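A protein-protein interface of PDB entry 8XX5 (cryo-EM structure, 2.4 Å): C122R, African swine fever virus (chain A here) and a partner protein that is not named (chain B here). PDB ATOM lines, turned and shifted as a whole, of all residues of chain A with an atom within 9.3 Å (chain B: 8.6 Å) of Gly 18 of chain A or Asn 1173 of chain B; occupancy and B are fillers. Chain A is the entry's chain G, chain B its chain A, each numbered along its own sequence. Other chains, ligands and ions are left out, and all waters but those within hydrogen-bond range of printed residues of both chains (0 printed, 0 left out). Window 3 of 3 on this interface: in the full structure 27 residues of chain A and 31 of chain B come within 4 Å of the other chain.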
ATOM      1  N   ARG A  13       6.415  36.335 -35.887  1.00  0.00           N
ATOM      2  CA  ARG A  13       5.143  35.628 -35.790  1.00  0.00           C
ATOM      3  C   ARG A  13       3.978  36.548 -35.443  1.00  0.00           C
ATOM      4  O   ARG A  13       2.978  36.566 -36.166  1.00  0.00           O
ATOM      5  CB  ARG A  13       5.267  34.498 -34.763  1.00  0.00           C
ATOM      6  CG  ARG A  13       5.563  33.145 -35.394  1.00  0.00           C
ATOM      7  CD  ARG A  13       6.136  32.161 -34.378  1.00  0.00           C
ATOM      8  NE  ARG A  13       6.083  30.770 -34.820  1.00  0.00           N
ATOM      9  CZ  ARG A  13       4.977  30.106 -35.131  1.00  0.00           C
ATOM     10  NH1 ARG A  13       3.779  30.653 -35.010  1.00  0.00           N
ATOM     11  NH2 ARG A  13       5.075  28.852 -35.562  1.00  0.00           N
ATOM     12  N   THR A  14       4.081  37.300 -34.346  1.00  0.00           N
ATOM     13  CA  THR A  14       3.165  38.398 -34.007  1.00  0.00           C
ATOM     14  C   THR A  14       1.694  37.986 -34.130  1.00  0.00           C
ATOM     15  O   THR A  14       0.948  38.467 -34.983  1.00  0.00           O
ATOM     16  CB  THR A  14       3.453  39.637 -34.864  1.00  0.00           C
ATOM     17  OG1 THR A  14       3.440  39.289 -36.255  1.00  0.00           O
ATOM     18  CG2 THR A  14       4.801  40.236 -34.498  1.00  0.00           C
ATOM     19  N   TYR A  15       1.297  37.069 -33.250  1.00  0.00           N
ATOM     20  CA  TYR A  15      -0.095  36.631 -33.176  1.00  0.00           C
ATOM     21  C   TYR A  15      -0.975  37.813 -32.788  1.00  0.00           C
ATOM     22  O   TYR A  15      -0.896  38.309 -31.660  1.00  0.00           O
ATOM     23  CB  TYR A  15      -0.246  35.500 -32.162  1.00  0.00           C
ATOM     24  CG  TYR A  15       0.882  34.494 -32.157  1.00  0.00           C
ATOM     25  CD1 TYR A  15       2.047  34.730 -31.438  1.00  0.00           C
ATOM     26  CD2 TYR A  15       0.780  33.305 -32.864  1.00  0.00           C
ATOM     27  CE1 TYR A  15       3.076  33.816 -31.428  1.00  0.00           C
ATOM     28  CE2 TYR A  15       1.807  32.383 -32.859  1.00  0.00           C
ATOM     29  CZ  TYR A  15       2.952  32.645 -32.139  1.00  0.00           C
ATOM     30  OH  TYR A  15       3.977  31.731 -32.130  1.00  0.00           O
ATOM     31  N   VAL A  16      -1.812  38.276 -33.717  1.00  0.00           N
ATOM     32  CA  VAL A  16      -2.657  39.438 -33.463  1.00  0.00           C
ATOM     33  C   VAL A  16      -4.124  39.116 -33.730  1.00  0.00           C
ATOM     34  O   VAL A  16      -4.976  39.280 -32.850  1.00  0.00           O
ATOM     35  CB  VAL A  16      -2.209  40.645 -34.308  1.00  0.00           C
ATOM     36  CG1 VAL A  16      -3.166  41.810 -34.114  1.00  0.00           C
ATOM     37  CG2 VAL A  16      -0.790  41.055 -33.942  1.00  0.00           C
ATOM     38  N   ASP A  17      -4.423  38.655 -34.940  1.00  0.00           N
ATOM     39  CA  ASP A  17      -5.798  38.489 -35.414  1.00  0.00           C
ATOM     40  C   ASP A  17      -6.421  37.159 -35.019  1.00  0.00           C
ATOM     41  O   ASP A  17      -7.365  36.726 -35.697  1.00  0.00           O
ATOM     42  CB  ASP A  17      -5.841  38.649 -36.934  1.00  0.00           C
ATOM     43  CG  ASP A  17      -7.138  39.266 -37.420  1.00  0.00           C
ATOM     44  OD1 ASP A  17      -7.763  40.023 -36.648  1.00  0.00           O
ATOM     45  OD2 ASP A  17      -7.532  38.994 -38.573  1.00  0.00           O
ATOM     46  N   GLY A  18      -5.957  36.486 -33.970  1.00  0.00           N
ATOM     47  CA  GLY A  18      -6.424  35.144 -33.697  1.00  0.00           C
ATOM     48  C   GLY A  18      -5.710  34.074 -34.484  1.00  0.00           C
ATOM     49  O   GLY A  18      -6.069  32.899 -34.379  1.00  0.00           O
ATOM     50  N   ASN A  19      -4.714  34.455 -35.281  1.00  0.00           N
ATOM     51  CA  ASN A  19      -3.878  33.529 -36.027  1.00  0.00           C
ATOM     52  C   ASN A  19      -2.503  34.163 -36.198  1.00  0.00           C
ATOM     53  O   ASN A  19      -2.240  35.267 -35.711  1.00  0.00           O
ATOM     54  CB  ASN A  19      -4.512  33.169 -37.374  1.00  0.00           C
ATOM     55  CG  ASN A  19      -4.703  34.376 -38.267  1.00  0.00           C
ATOM     56  OD1 ASN A  19      -4.720  35.514 -37.798  1.00  0.00           O
ATOM     57  ND2 ASN A  19      -4.849  34.134 -39.564  1.00  0.00           N
ATOM     58  N   ILE A  20      -1.621  33.458 -36.892  1.00  0.00           N
ATOM     59  CA  ILE A  20      -0.246  33.906 -37.080  1.00  0.00           C
ATOM     60  C   ILE A  20      -0.196  34.839 -38.280  1.00  0.00           C
ATOM     61  O   ILE A  20      -0.713  34.514 -39.355  1.00  0.00           O
ATOM     62  CB  ILE A  20       0.717  32.718 -37.268  1.00  0.00           C
ATOM     63  CG1 ILE A  20       0.451  31.580 -36.271  1.00  0.00           C
ATOM     64  CG2 ILE A  20       2.161  33.185 -37.152  1.00  0.00           C
ATOM     65  CD1 ILE A  20      -0.669  30.616 -36.654  1.00  0.00           C
ATOM     66  N   ILE A  21       0.421  36.003 -38.097  1.00  0.00           N
ATOM     67  CA  ILE A  21       0.636  36.970 -39.168  1.00  0.00           C
ATOM     68  C   ILE A  21       2.144  37.130 -39.303  1.00  0.00           C
ATOM     69  O   ILE A  21       2.776  37.851 -38.522  1.00  0.00           O
ATOM     70  CB  ILE A  21      -0.047  38.313 -38.888  1.00  0.00           C
ATOM     71  CG1 ILE A  21      -1.569  38.166 -38.929  1.00  0.00           C
ATOM     72  CG2 ILE A  21       0.387  39.354 -39.907  1.00  0.00           C
ATOM     73  CD1 ILE A  21      -2.074  37.338 -40.083  1.00  0.00           C
ATOM     74  N   GLN A  31       0.354  35.409 -44.033  1.00  0.00           N
ATOM     75  CA  GLN A  31      -0.729  34.752 -43.306  1.00  0.00           C
ATOM     76  C   GLN A  31      -0.239  33.409 -42.784  1.00  0.00           C
ATOM     77  O   GLN A  31       0.211  33.311 -41.637  1.00  0.00           O
ATOM     78  CB  GLN A  31      -1.975  34.581 -44.187  1.00  0.00           C
ATOM     79  CG  GLN A  31      -3.267  34.306 -43.431  1.00  0.00           C
ATOM     80  CD  GLN A  31      -3.702  35.468 -42.563  1.00  0.00           C
ATOM     81  OE1 GLN A  31      -4.185  35.275 -41.448  1.00  0.00           O
ATOM     82  NE2 GLN A  31      -3.538  36.683 -43.073  1.00  0.00           N
ATOM     83  N   ASP A  33      -1.508  29.824 -42.279  1.00  0.00           N
ATOM     84  CA  ASP A  33      -2.155  29.051 -41.232  1.00  0.00           C
ATOM     85  C   ASP A  33      -1.750  27.577 -41.320  1.00  0.00           C
ATOM     86  O   ASP A  33      -0.953  27.172 -42.171  1.00  0.00           O
ATOM     87  CB  ASP A  33      -3.676  29.201 -41.326  1.00  0.00           C
ATOM     88  CG  ASP A  33      -4.379  28.908 -40.013  1.00  0.00           C
ATOM     89  OD1 ASP A  33      -3.685  28.717 -38.991  1.00  0.00           O
ATOM     90  OD2 ASP A  33      -5.627  28.871 -40.003  1.00  0.00           O
ATOM     91  N   LEU A  37       1.447  26.135 -36.467  1.00  0.00           N
ATOM     92  CA  LEU A  37       0.835  26.363 -35.163  1.00  0.00           C
ATOM     93  C   LEU A  37       1.752  25.971 -34.011  1.00  0.00           C
ATOM     94  O   LEU A  37       1.396  26.206 -32.852  1.00  0.00           O
ATOM     95  CB  LEU A  37      -0.489  25.604 -35.057  1.00  0.00           C
ATOM     96  CG  LEU A  37      -1.745  26.331 -35.547  1.00  0.00           C
ATOM     97  CD1 LEU A  37      -1.883  27.668 -34.856  1.00  0.00           C
ATOM     98  CD2 LEU A  37      -1.725  26.525 -37.043  1.00  0.00           C
ATOM     99  N   VAL A  39       4.703  26.748 -31.761  1.00  0.00           N
ATOM    100  CA  VAL A  39       5.483  27.925 -31.394  1.00  0.00           C
ATOM    101  C   VAL A  39       6.749  27.546 -30.635  1.00  0.00           C
ATOM    102  O   VAL A  39       7.828  28.072 -30.919  1.00  0.00           O
ATOM    103  CB  VAL A  39       4.608  28.912 -30.590  1.00  0.00           C
ATOM    104  CG1 VAL A  39       3.482  28.184 -29.888  1.00  0.00           C
ATOM    105  CG2 VAL A  39       5.447  29.700 -29.592  1.00  0.00           C
ATOM    106  N   LEU B1131       3.956  23.612 -27.354  1.00  0.00           N
ATOM    107  CA  LEU B1131       2.878  24.568 -27.151  1.00  0.00           C
ATOM    108  C   LEU B1131       2.288  24.962 -28.500  1.00  0.00           C
ATOM    109  O   LEU B1131       3.013  25.112 -29.489  1.00  0.00           O
ATOM    110  CB  LEU B1131       3.384  25.801 -26.403  1.00  0.00           C
ATOM    111  CG  LEU B1131       2.503  27.051 -26.396  1.00  0.00           C
ATOM    112  CD1 LEU B1131       1.373  26.908 -25.394  1.00  0.00           C
ATOM    113  CD2 LEU B1131       3.332  28.285 -26.090  1.00  0.00           C
ATOM    114  N   LEU B1132       0.967  25.106 -28.543  1.00  0.00           N
ATOM    115  CA  LEU B1132       0.251  25.326 -29.790  1.00  0.00           C
ATOM    116  C   LEU B1132      -0.696  26.508 -29.651  1.00  0.00           C
ATOM    117  O   LEU B1132      -1.195  26.795 -28.561  1.00  0.00           O
ATOM    118  CB  LEU B1132      -0.533  24.075 -30.203  1.00  0.00           C
ATOM    119  CG  LEU B1132       0.276  22.781 -30.319  1.00  0.00           C
ATOM    120  CD1 LEU B1132      -0.628  21.604 -30.645  1.00  0.00           C
ATOM    121  CD2 LEU B1132       1.373  22.922 -31.363  1.00  0.00           C
ATOM    122  N   TYR B1133      -0.942  27.185 -30.774  1.00  0.00           N
ATOM    123  CA  TYR B1133      -1.858  28.317 -30.853  1.00  0.00           C
ATOM    124  C   TYR B1133      -3.268  27.889 -31.254  1.00  0.00           C
ATOM    125  O   TYR B1133      -3.992  28.656 -31.901  1.00  0.00           O
ATOM    126  CB  TYR B1133      -1.299  29.357 -31.826  1.00  0.00           C
ATOM    127  CG  TYR B1133      -1.877  30.752 -31.711  1.00  0.00           C
ATOM    128  CD1 TYR B1133      -1.606  31.548 -30.608  1.00  0.00           C
ATOM    129  CD2 TYR B1133      -2.665  31.284 -32.724  1.00  0.00           C
ATOM    130  CE1 TYR B1133      -2.123  32.826 -30.506  1.00  0.00           C
ATOM    131  CE2 TYR B1133      -3.184  32.560 -32.630  1.00  0.00           C
ATOM    132  CZ  TYR B1133      -2.910  33.326 -31.520  1.00  0.00           C
ATOM    133  OH  TYR B1133      -3.426  34.597 -31.424  1.00  0.00           O
ATOM    134  N   GLU B1134      -3.673  26.677 -30.879  1.00  0.00           N
ATOM    135  CA  GLU B1134      -4.919  26.074 -31.328  1.00  0.00           C
ATOM    136  C   GLU B1134      -5.917  25.960 -30.182  1.00  0.00           C
ATOM    137  O   GLU B1134      -5.581  25.475 -29.098  1.00  0.00           O
ATOM    138  CB  GLU B1134      -4.659  24.683 -31.905  1.00  0.00           C
ATOM    139  CG  GLU B1134      -3.401  24.581 -32.738  1.00  0.00           C
ATOM    140  CD  GLU B1134      -2.914  23.155 -32.858  1.00  0.00           C
ATOM    141  OE1 GLU B1134      -3.618  22.246 -32.368  1.00  0.00           O
ATOM    142  OE2 GLU B1134      -1.834  22.939 -33.445  1.00  0.00           O
ATOM    143  N   THR B1135      -7.148  26.386 -30.437  1.00  0.00           N
ATOM    144  CA  THR B1135      -8.241  26.236 -29.493  1.00  0.00           C
ATOM    145  C   THR B1135      -8.946  24.901 -29.737  1.00  0.00           C
ATOM    146  O   THR B1135      -8.544  24.108 -30.593  1.00  0.00           O
ATOM    147  CB  THR B1135      -9.204  27.421 -29.612  1.00  0.00           C
ATOM    148  OG1 THR B1135     -10.370  27.176 -28.815  1.00  0.00           O
ATOM    149  CG2 THR B1135      -9.618  27.624 -31.061  1.00  0.00           C
ATOM    150  N   TYR B1136     -10.009  24.644 -28.977  1.00  0.00           N
ATOM    151  CA  TYR B1136     -10.784  23.422 -29.144  1.00  0.00           C
ATOM    152  C   TYR B1136     -12.207  23.654 -28.658  1.00  0.00           C
ATOM    153  O   TYR B1136     -12.438  24.470 -27.764  1.00  0.00           O
ATOM    154  CB  TYR B1136     -10.155  22.244 -28.388  1.00  0.00           C
ATOM    155  CG  TYR B1136     -10.882  20.937 -28.605  1.00  0.00           C
ATOM    156  CD1 TYR B1136     -11.134  20.464 -29.886  1.00  0.00           C
ATOM    157  CD2 TYR B1136     -11.330  20.182 -27.529  1.00  0.00           C
ATOM    158  CE1 TYR B1136     -11.809  19.275 -30.090  1.00  0.00           C
ATOM    159  CE2 TYR B1136     -12.003  18.990 -27.723  1.00  0.00           C
ATOM    160  CZ  TYR B1136     -12.239  18.542 -29.006  1.00  0.00           C
ATOM    161  OH  TYR B1136     -12.906  17.355 -29.207  1.00  0.00           O
ATOM    162  N   VAL B1143      -6.386  25.423 -35.095  1.00  0.00           N
ATOM    163  CA  VAL B1143      -7.060  24.176 -35.425  1.00  0.00           C
ATOM    164  C   VAL B1143      -6.227  22.989 -34.966  1.00  0.00           C
ATOM    165  O   VAL B1143      -6.492  22.414 -33.911  1.00  0.00           O
ATOM    166  CB  VAL B1143      -7.357  24.082 -36.930  1.00  0.00           C
ATOM    167  CG1 VAL B1143      -8.168  22.831 -37.234  1.00  0.00           C
ATOM    168  CG2 VAL B1143      -8.093  25.328 -37.399  1.00  0.00           C
ATOM    169  N   ASP B1170     -14.341  29.105 -22.187  1.00  0.00           N
ATOM    170  CA  ASP B1170     -13.331  30.153 -22.136  1.00  0.00           C
ATOM    171  C   ASP B1170     -12.010  29.636 -22.690  1.00  0.00           C
ATOM    172  O   ASP B1170     -10.936  30.094 -22.288  1.00  0.00           O
ATOM    173  CB  ASP B1170     -13.155  30.701 -20.718  1.00  0.00           C
ATOM    174  CG  ASP B1170     -12.864  29.620 -19.704  1.00  0.00           C
ATOM    175  OD1 ASP B1170     -13.220  28.453 -19.959  1.00  0.00           O
ATOM    176  OD2 ASP B1170     -12.291  29.942 -18.643  1.00  0.00           O
ATOM    177  N   ILE B1171     -12.078  28.663 -23.593  1.00  0.00           N
ATOM    178  CA  ILE B1171     -10.887  28.033 -24.150  1.00  0.00           C
ATOM    179  C   ILE B1171     -10.210  29.005 -25.107  1.00  0.00           C
ATOM    180  O   ILE B1171     -10.852  29.569 -26.001  1.00  0.00           O
ATOM    181  CB  ILE B1171     -11.252  26.714 -24.851  1.00  0.00           C
ATOM    182  CG1 ILE B1171     -10.080  26.199 -25.687  1.00  0.00           C
ATOM    183  CG2 ILE B1171     -12.506  26.887 -25.700  1.00  0.00           C
ATOM    184  CD1 ILE B1171      -8.855  25.875 -24.875  1.00  0.00           C
ATOM    185  N   ALA B1172      -8.909  29.202 -24.921  1.00  0.00           N
ATOM    186  CA  ALA B1172      -8.136  30.126 -25.731  1.00  0.00           C
ATOM    187  C   ALA B1172      -7.268  29.359 -26.724  1.00  0.00           C
ATOM    188  O   ALA B1172      -7.332  28.132 -26.838  1.00  0.00           O
ATOM    189  CB  ALA B1172      -7.289  31.032 -24.840  1.00  0.00           C
ATOM    190  N   ASN B1173      -6.441  30.105 -27.458  1.00  0.00           N
ATOM    191  CA  ASN B1173      -5.624  29.495 -28.500  1.00  0.00           C
ATOM    192  C   ASN B1173      -4.449  28.716 -27.920  1.00  0.00           C
ATOM    193  O   ASN B1173      -4.086  27.663 -28.452  1.00  0.00           O
ATOM    194  CB  ASN B1173      -5.124  30.570 -29.463  1.00  0.00           C
ATOM    195  CG  ASN B1173      -6.200  31.033 -30.424  1.00  0.00           C
ATOM    196  OD1 ASN B1173      -7.326  31.320 -30.019  1.00  0.00           O
ATOM    197  ND2 ASN B1173      -5.861  31.102 -31.705  1.00  0.00           N
ATOM    198  N   TRP B1174      -3.845  29.208 -26.844  1.00  0.00           N
ATOM    199  CA  TRP B1174      -2.631  28.594 -26.326  1.00  0.00           C
ATOM    200  C   TRP B1174      -2.927  27.246 -25.674  1.00  0.00           C
ATOM    201  O   TRP B1174      -3.922  27.084 -24.964  1.00  0.00           O
ATOM    202  CB  TRP B1174      -1.956  29.534 -25.332  1.00  0.00           C
ATOM    203  CG  TRP B1174      -1.540  30.842 -25.945  1.00  0.00           C
ATOM    204  CD1 TRP B1174      -2.114  32.064 -25.741  1.00  0.00           C
ATOM    205  CD2 TRP B1174      -0.461  31.056 -26.862  1.00  0.00           C
ATOM    206  NE1 TRP B1174      -1.460  33.024 -26.472  1.00  0.00           N
ATOM    207  CE2 TRP B1174      -0.441  32.431 -27.169  1.00  0.00           C
ATOM    208  CE3 TRP B1174       0.491  30.220 -27.453  1.00  0.00           C
ATOM    209  CZ2 TRP B1174       0.492  32.987 -28.041  1.00  0.00           C
ATOM    210  CZ3 TRP B1174       1.416  30.775 -28.317  1.00  0.00           C
ATOM    211  CH2 TRP B1174       1.410  32.145 -28.603  1.00  0.00           C
ATOM    212  N   CYS B1175      -2.049  26.271 -25.927  1.00  0.00           N
ATOM    213  CA  CYS B1175      -2.177  24.934 -25.357  1.00  0.00           C
ATOM    214  C   CYS B1175      -0.872  24.155 -25.493  1.00  0.00           C
ATOM    215  O   CYS B1175      -0.185  24.263 -26.513  1.00  0.00           O
ATOM    216  CB  CYS B1175      -3.331  24.175 -26.021  1.00  0.00           C
ATOM    217  SG  CYS B1175      -2.886  23.128 -27.428  1.00  0.00           S
ATOM    218  N   ILE B1176      -0.505  23.385 -24.465  1.00  0.00           N
ATOM    219  CA  ILE B1176       0.693  22.551 -24.503  1.00  0.00           C
ATOM    220  C   ILE B1176       0.286  21.142 -24.900  1.00  0.00           C
ATOM    221  O   ILE B1176      -0.791  20.663 -24.525  1.00  0.00           O
ATOM    222  CB  ILE B1176       1.458  22.518 -23.161  1.00  0.00           C
ATOM    223  CG1 ILE B1176       1.553  23.886 -22.484  1.00  0.00           C
ATOM    224  CG2 ILE B1176       2.864  21.972 -23.359  1.00  0.00           C
ATOM    225  CD1 ILE B1176       0.374  24.252 -21.640  1.00  0.00           C
ATOM    226  N   ILE B1225      -2.637  20.002 -22.590  1.00  0.00           N
ATOM    227  CA  ILE B1225      -3.174  20.948 -21.621  1.00  0.00           C
ATOM    228  C   ILE B1225      -3.589  22.203 -22.371  1.00  0.00           C
ATOM    229  O   ILE B1225      -2.746  22.904 -22.942  1.00  0.00           O
ATOM    230  CB  ILE B1225      -2.153  21.276 -20.521  1.00  0.00           C
ATOM    231  CG1 ILE B1225      -1.820  20.027 -19.705  1.00  0.00           C
ATOM    232  CG2 ILE B1225      -2.677  22.376 -19.624  1.00  0.00           C
ATOM    233  CD1 ILE B1225      -0.466  20.075 -19.055  1.00  0.00           C
ATOM    234  N   TYR B1226      -4.888  22.486 -22.366  1.00  0.00           N
ATOM    235  CA  TYR B1226      -5.430  23.660 -23.035  1.00  0.00           C
ATOM    236  C   TYR B1226      -5.591  24.787 -22.023  1.00  0.00           C
ATOM    237  O   TYR B1226      -6.143  24.581 -20.938  1.00  0.00           O
ATOM    238  CB  TYR B1226      -6.770  23.329 -23.692  1.00  0.00           C
ATOM    239  CG  TYR B1226      -6.647  22.589 -25.007  1.00  0.00           C
ATOM    240  CD1 TYR B1226      -6.514  21.207 -25.040  1.00  0.00           C
ATOM    241  CD2 TYR B1226      -6.668  23.273 -26.215  1.00  0.00           C
ATOM    242  CE1 TYR B1226      -6.403  20.528 -26.240  1.00  0.00           C
ATOM    243  CE2 TYR B1226      -6.555  22.604 -27.418  1.00  0.00           C
ATOM    244  CZ  TYR B1226      -6.422  21.232 -27.426  1.00  0.00           C
ATOM    245  OH  TYR B1226      -6.310  20.564 -28.623  1.00  0.00           O
ATOM    246  N   LEU B1227      -5.101  25.973 -22.376  1.00  0.00           N
ATOM    247  CA  LEU B1227      -5.154  27.107 -21.467  1.00  0.00           C
ATOM    248  C   LEU B1227      -6.489  27.832 -21.593  1.00  0.00           C
ATOM    249  O   LEU B1227      -7.345  27.496 -22.416  1.00  0.00           O
ATOM    250  CB  LEU B1227      -4.004  28.084 -21.718  1.00  0.00           C
ATOM    251  CG  LEU B1227      -2.547  27.712 -21.422  1.00  0.00           C
ATOM    252  CD1 LEU B1227      -2.118  26.494 -22.188  1.00  0.00           C
ATOM    253  CD2 LEU B1227      -1.611  28.870 -21.712  1.00  0.00           C
ATOM    254  N   ARG B1228      -6.658  28.846 -20.752  1.00  0.00           N
ATOM    255  CA  ARG B1228      -7.841  29.690 -20.744  1.00  0.00           C
ATOM    256  C   ARG B1228      -7.379  31.137 -20.660  1.00  0.00           C
ATOM    257  O   ARG B1228      -6.266  31.428 -20.215  1.00  0.00           O
ATOM    258  CB  ARG B1228      -8.771  29.340 -19.574  1.00  0.00           C
ATOM    259  CG  ARG B1228      -8.879  27.845 -19.284  1.00  0.00           C
ATOM    260  CD  ARG B1228     -10.274  27.448 -18.841  1.00  0.00           C
ATOM    261  NE  ARG B1228     -10.486  27.723 -17.425  1.00  0.00           N
ATOM    262  CZ  ARG B1228     -11.608  27.462 -16.769  1.00  0.00           C
ATOM    263  NH1 ARG B1228     -12.649  26.912 -17.372  1.00  0.00           N
ATOM    264  NH2 ARG B1228     -11.689  27.762 -15.476  1.00  0.00           N
ATOM    265  N   GLU B1229      -8.240  32.056 -21.099  1.00  0.00           N
ATOM    266  CA  GLU B1229      -7.896  33.470 -21.019  1.00  0.00           C
ATOM    267  C   GLU B1229      -7.854  33.977 -19.584  1.00  0.00           C
ATOM    268  O   GLU B1229      -7.380  35.094 -19.351  1.00  0.00           O
ATOM    269  CB  GLU B1229      -8.876  34.315 -21.837  1.00  0.00           C
ATOM    270  CG  GLU B1229      -9.178  33.769 -23.221  1.00  0.00           C
ATOM    271  CD  GLU B1229     -10.406  32.885 -23.239  1.00  0.00           C
ATOM    272  OE1 GLU B1229     -11.159  32.895 -22.243  1.00  0.00           O
ATOM    273  OE2 GLU B1229     -10.616  32.181 -24.249  1.00  0.00           O
ATOM    274  N   PHE B1232      -4.397  34.514 -19.049  1.00  0.00           N
ATOM    275  CA  PHE B1232      -3.930  35.689 -19.778  1.00  0.00           C
ATOM    276  C   PHE B1232      -4.556  36.963 -19.225  1.00  0.00           C
ATOM    277  O   PHE B1232      -4.161  38.072 -19.601  1.00  0.00           O
ATOM    278  CB  PHE B1232      -4.236  35.549 -21.272  1.00  0.00           C
ATOM    279  CG  PHE B1232      -3.982  34.172 -21.825  1.00  0.00           C
ATOM    280  CD1 PHE B1232      -2.916  33.410 -21.377  1.00  0.00           C
ATOM    281  CD2 PHE B1232      -4.807  33.644 -22.799  1.00  0.00           C
ATOM    282  CE1 PHE B1232      -2.685  32.152 -21.880  1.00  0.00           C
ATOM    283  CE2 PHE B1232      -4.576  32.383 -23.307  1.00  0.00           C
ATOM    284  CZ  PHE B1232      -3.516  31.637 -22.846  1.00  0.00           C
ATOM    285  N   ASP B1243       1.884  38.132 -25.174  1.00  0.00           N
ATOM    286  CA  ASP B1243       1.037  36.972 -24.931  1.00  0.00           C
ATOM    287  C   ASP B1243       1.825  35.669 -25.034  1.00  0.00           C
ATOM    288  O   ASP B1243       1.658  34.758 -24.216  1.00  0.00           O
ATOM    289  CB  ASP B1243      -0.135  36.976 -25.918  1.00  0.00           C
ATOM    290  CG  ASP B1243      -1.342  36.218 -25.399  1.00  0.00           C
ATOM    291  OD1 ASP B1243      -1.168  35.337 -24.529  1.00  0.00           O
ATOM    292  OD2 ASP B1243      -2.467  36.502 -25.859  1.00  0.00           O
ATOM    293  N   ALA B1247       2.525  33.060 -22.025  1.00  0.00           N
ATOM    294  CA  ALA B1247       2.152  31.673 -22.264  1.00  0.00           C
ATOM    295  C   ALA B1247       3.301  30.705 -22.017  1.00  0.00           C
ATOM    296  O   ALA B1247       3.090  29.656 -21.400  1.00  0.00           O
ATOM    297  CB  ALA B1247       1.635  31.502 -23.695  1.00  0.00           C
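O of Leu 37 of chain A sits at hydrogen-bond distance from N of Tyr 1133 of chain B. The backbone NH of Val 39 of chain A lies close to the backbone carbonyl oxygen of Leu 1131 of chain B. The backbone carbonyl oxygen (O) of Gly 18 of chain A sits at hydrogen-bond distance from the side-chain amide nitrogen (ND2) of Asn 1173 of chain B.
The backbone carbonyl oxygen (O) of Trp 1174 of chain B is in hydrogen-bond range of the backbone NH (N) of Leu 1227 of chain B, 3.1 Å away. The indole nitrogen of Trp 1174 of chain B lies within hydrogen-bond range of the side-chain carboxylate of Asp 1243 of chain B. ND2 of Asn 1173 of chain B sits at hydrogen-bond distance from O of Tyr 1133 of chain B. N of Glu 1134 of chain B lies within hydrogen-bond range of O of Asn 1173 of chain B, 2.7 Å away. The backbone NH (N) of Leu 1132 of chain B sits at hydrogen-bond distance from the backbone carbonyl oxygen (O) of Cys 1175 of chain B, 2.5 Å away. NH1 of Arg 13 of chain A sits at hydrogen-bond distance from OH of Tyr 15 of chain A (3.1 Å).
OH of Tyr 1133 of chain B touches CB of Tyr 15 of chain A, at 3.4 Å. CH2 of Trp 1174 of chain B touches CE1 of Tyr 15 of chain A (3.7 Å). Tyr 1133 of chain B touches Gly 18 of chain A (CE2 to O, 3.4 Å). N of Asn 19 of chain A touches CE2 of Tyr 1133 of chain B (3.6 Å). O of Leu 37 of chain A touches O of Leu 1131 of chain B, 3.9 Å away. O of Leu 37 of chain A touches CA of Leu 1132 of chain B, 3.4 Å away. CB of Leu 37 of chain A touches OE2 of Glu 1134 of chain B, at 3.4 Å. Val 39 of chain A touches Trp 1174 of chain B.
Of the printed residues of chain B, Tyr 15 of chain A touches Tyr 1133 and Trp 1174. Gly 18 of chain A touches just these residues of chain B: Tyr 1133 and Asn 1173. Of chain A, only Tyr 15 (3.4 Å), Gly 18 (3.4 Å), Asn 19 (3.6 Å) and Leu 37 (3.3 Å) come within 4 Å of Tyr 1133 of chain B. No residue of chain A comes within 4 Å of Ala 1172 of chain B. Asn 1173 of chain B touches one residue of chain A. Of the printed residues of chain A, Trp 1174 of chain B touches Tyr 15 (3.7 Å) and Val 39 (3.7 Å). The nearest residue of chain B that does not touch Gly 18 of chain A is Thr 1135 of chain B (7.2 Å). The nearest printed residue of chain B that does not touch Val 39 of chain A is Leu 1132 of chain B (4.2 Å).
Hydrophobic or aromatic side chains of chain B that line the printed part of chain A: Leu 1131, Leu 1132, Tyr 1133 and Trp 1174. Printed residues of chain A that touch a printed residue of chain B: Tyr 15, Gly 18, Asn 19, Leu 37 and Val 39. Hydrophobic or aromatic side chains of chain A that line the printed part of chain B: Tyr 15, Leu 37 and Val 39. Among the printed residues, no Asp or Glu carboxylate lies within 4 Å of a Lys or Arg side-chain nitrogen of the other chain.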
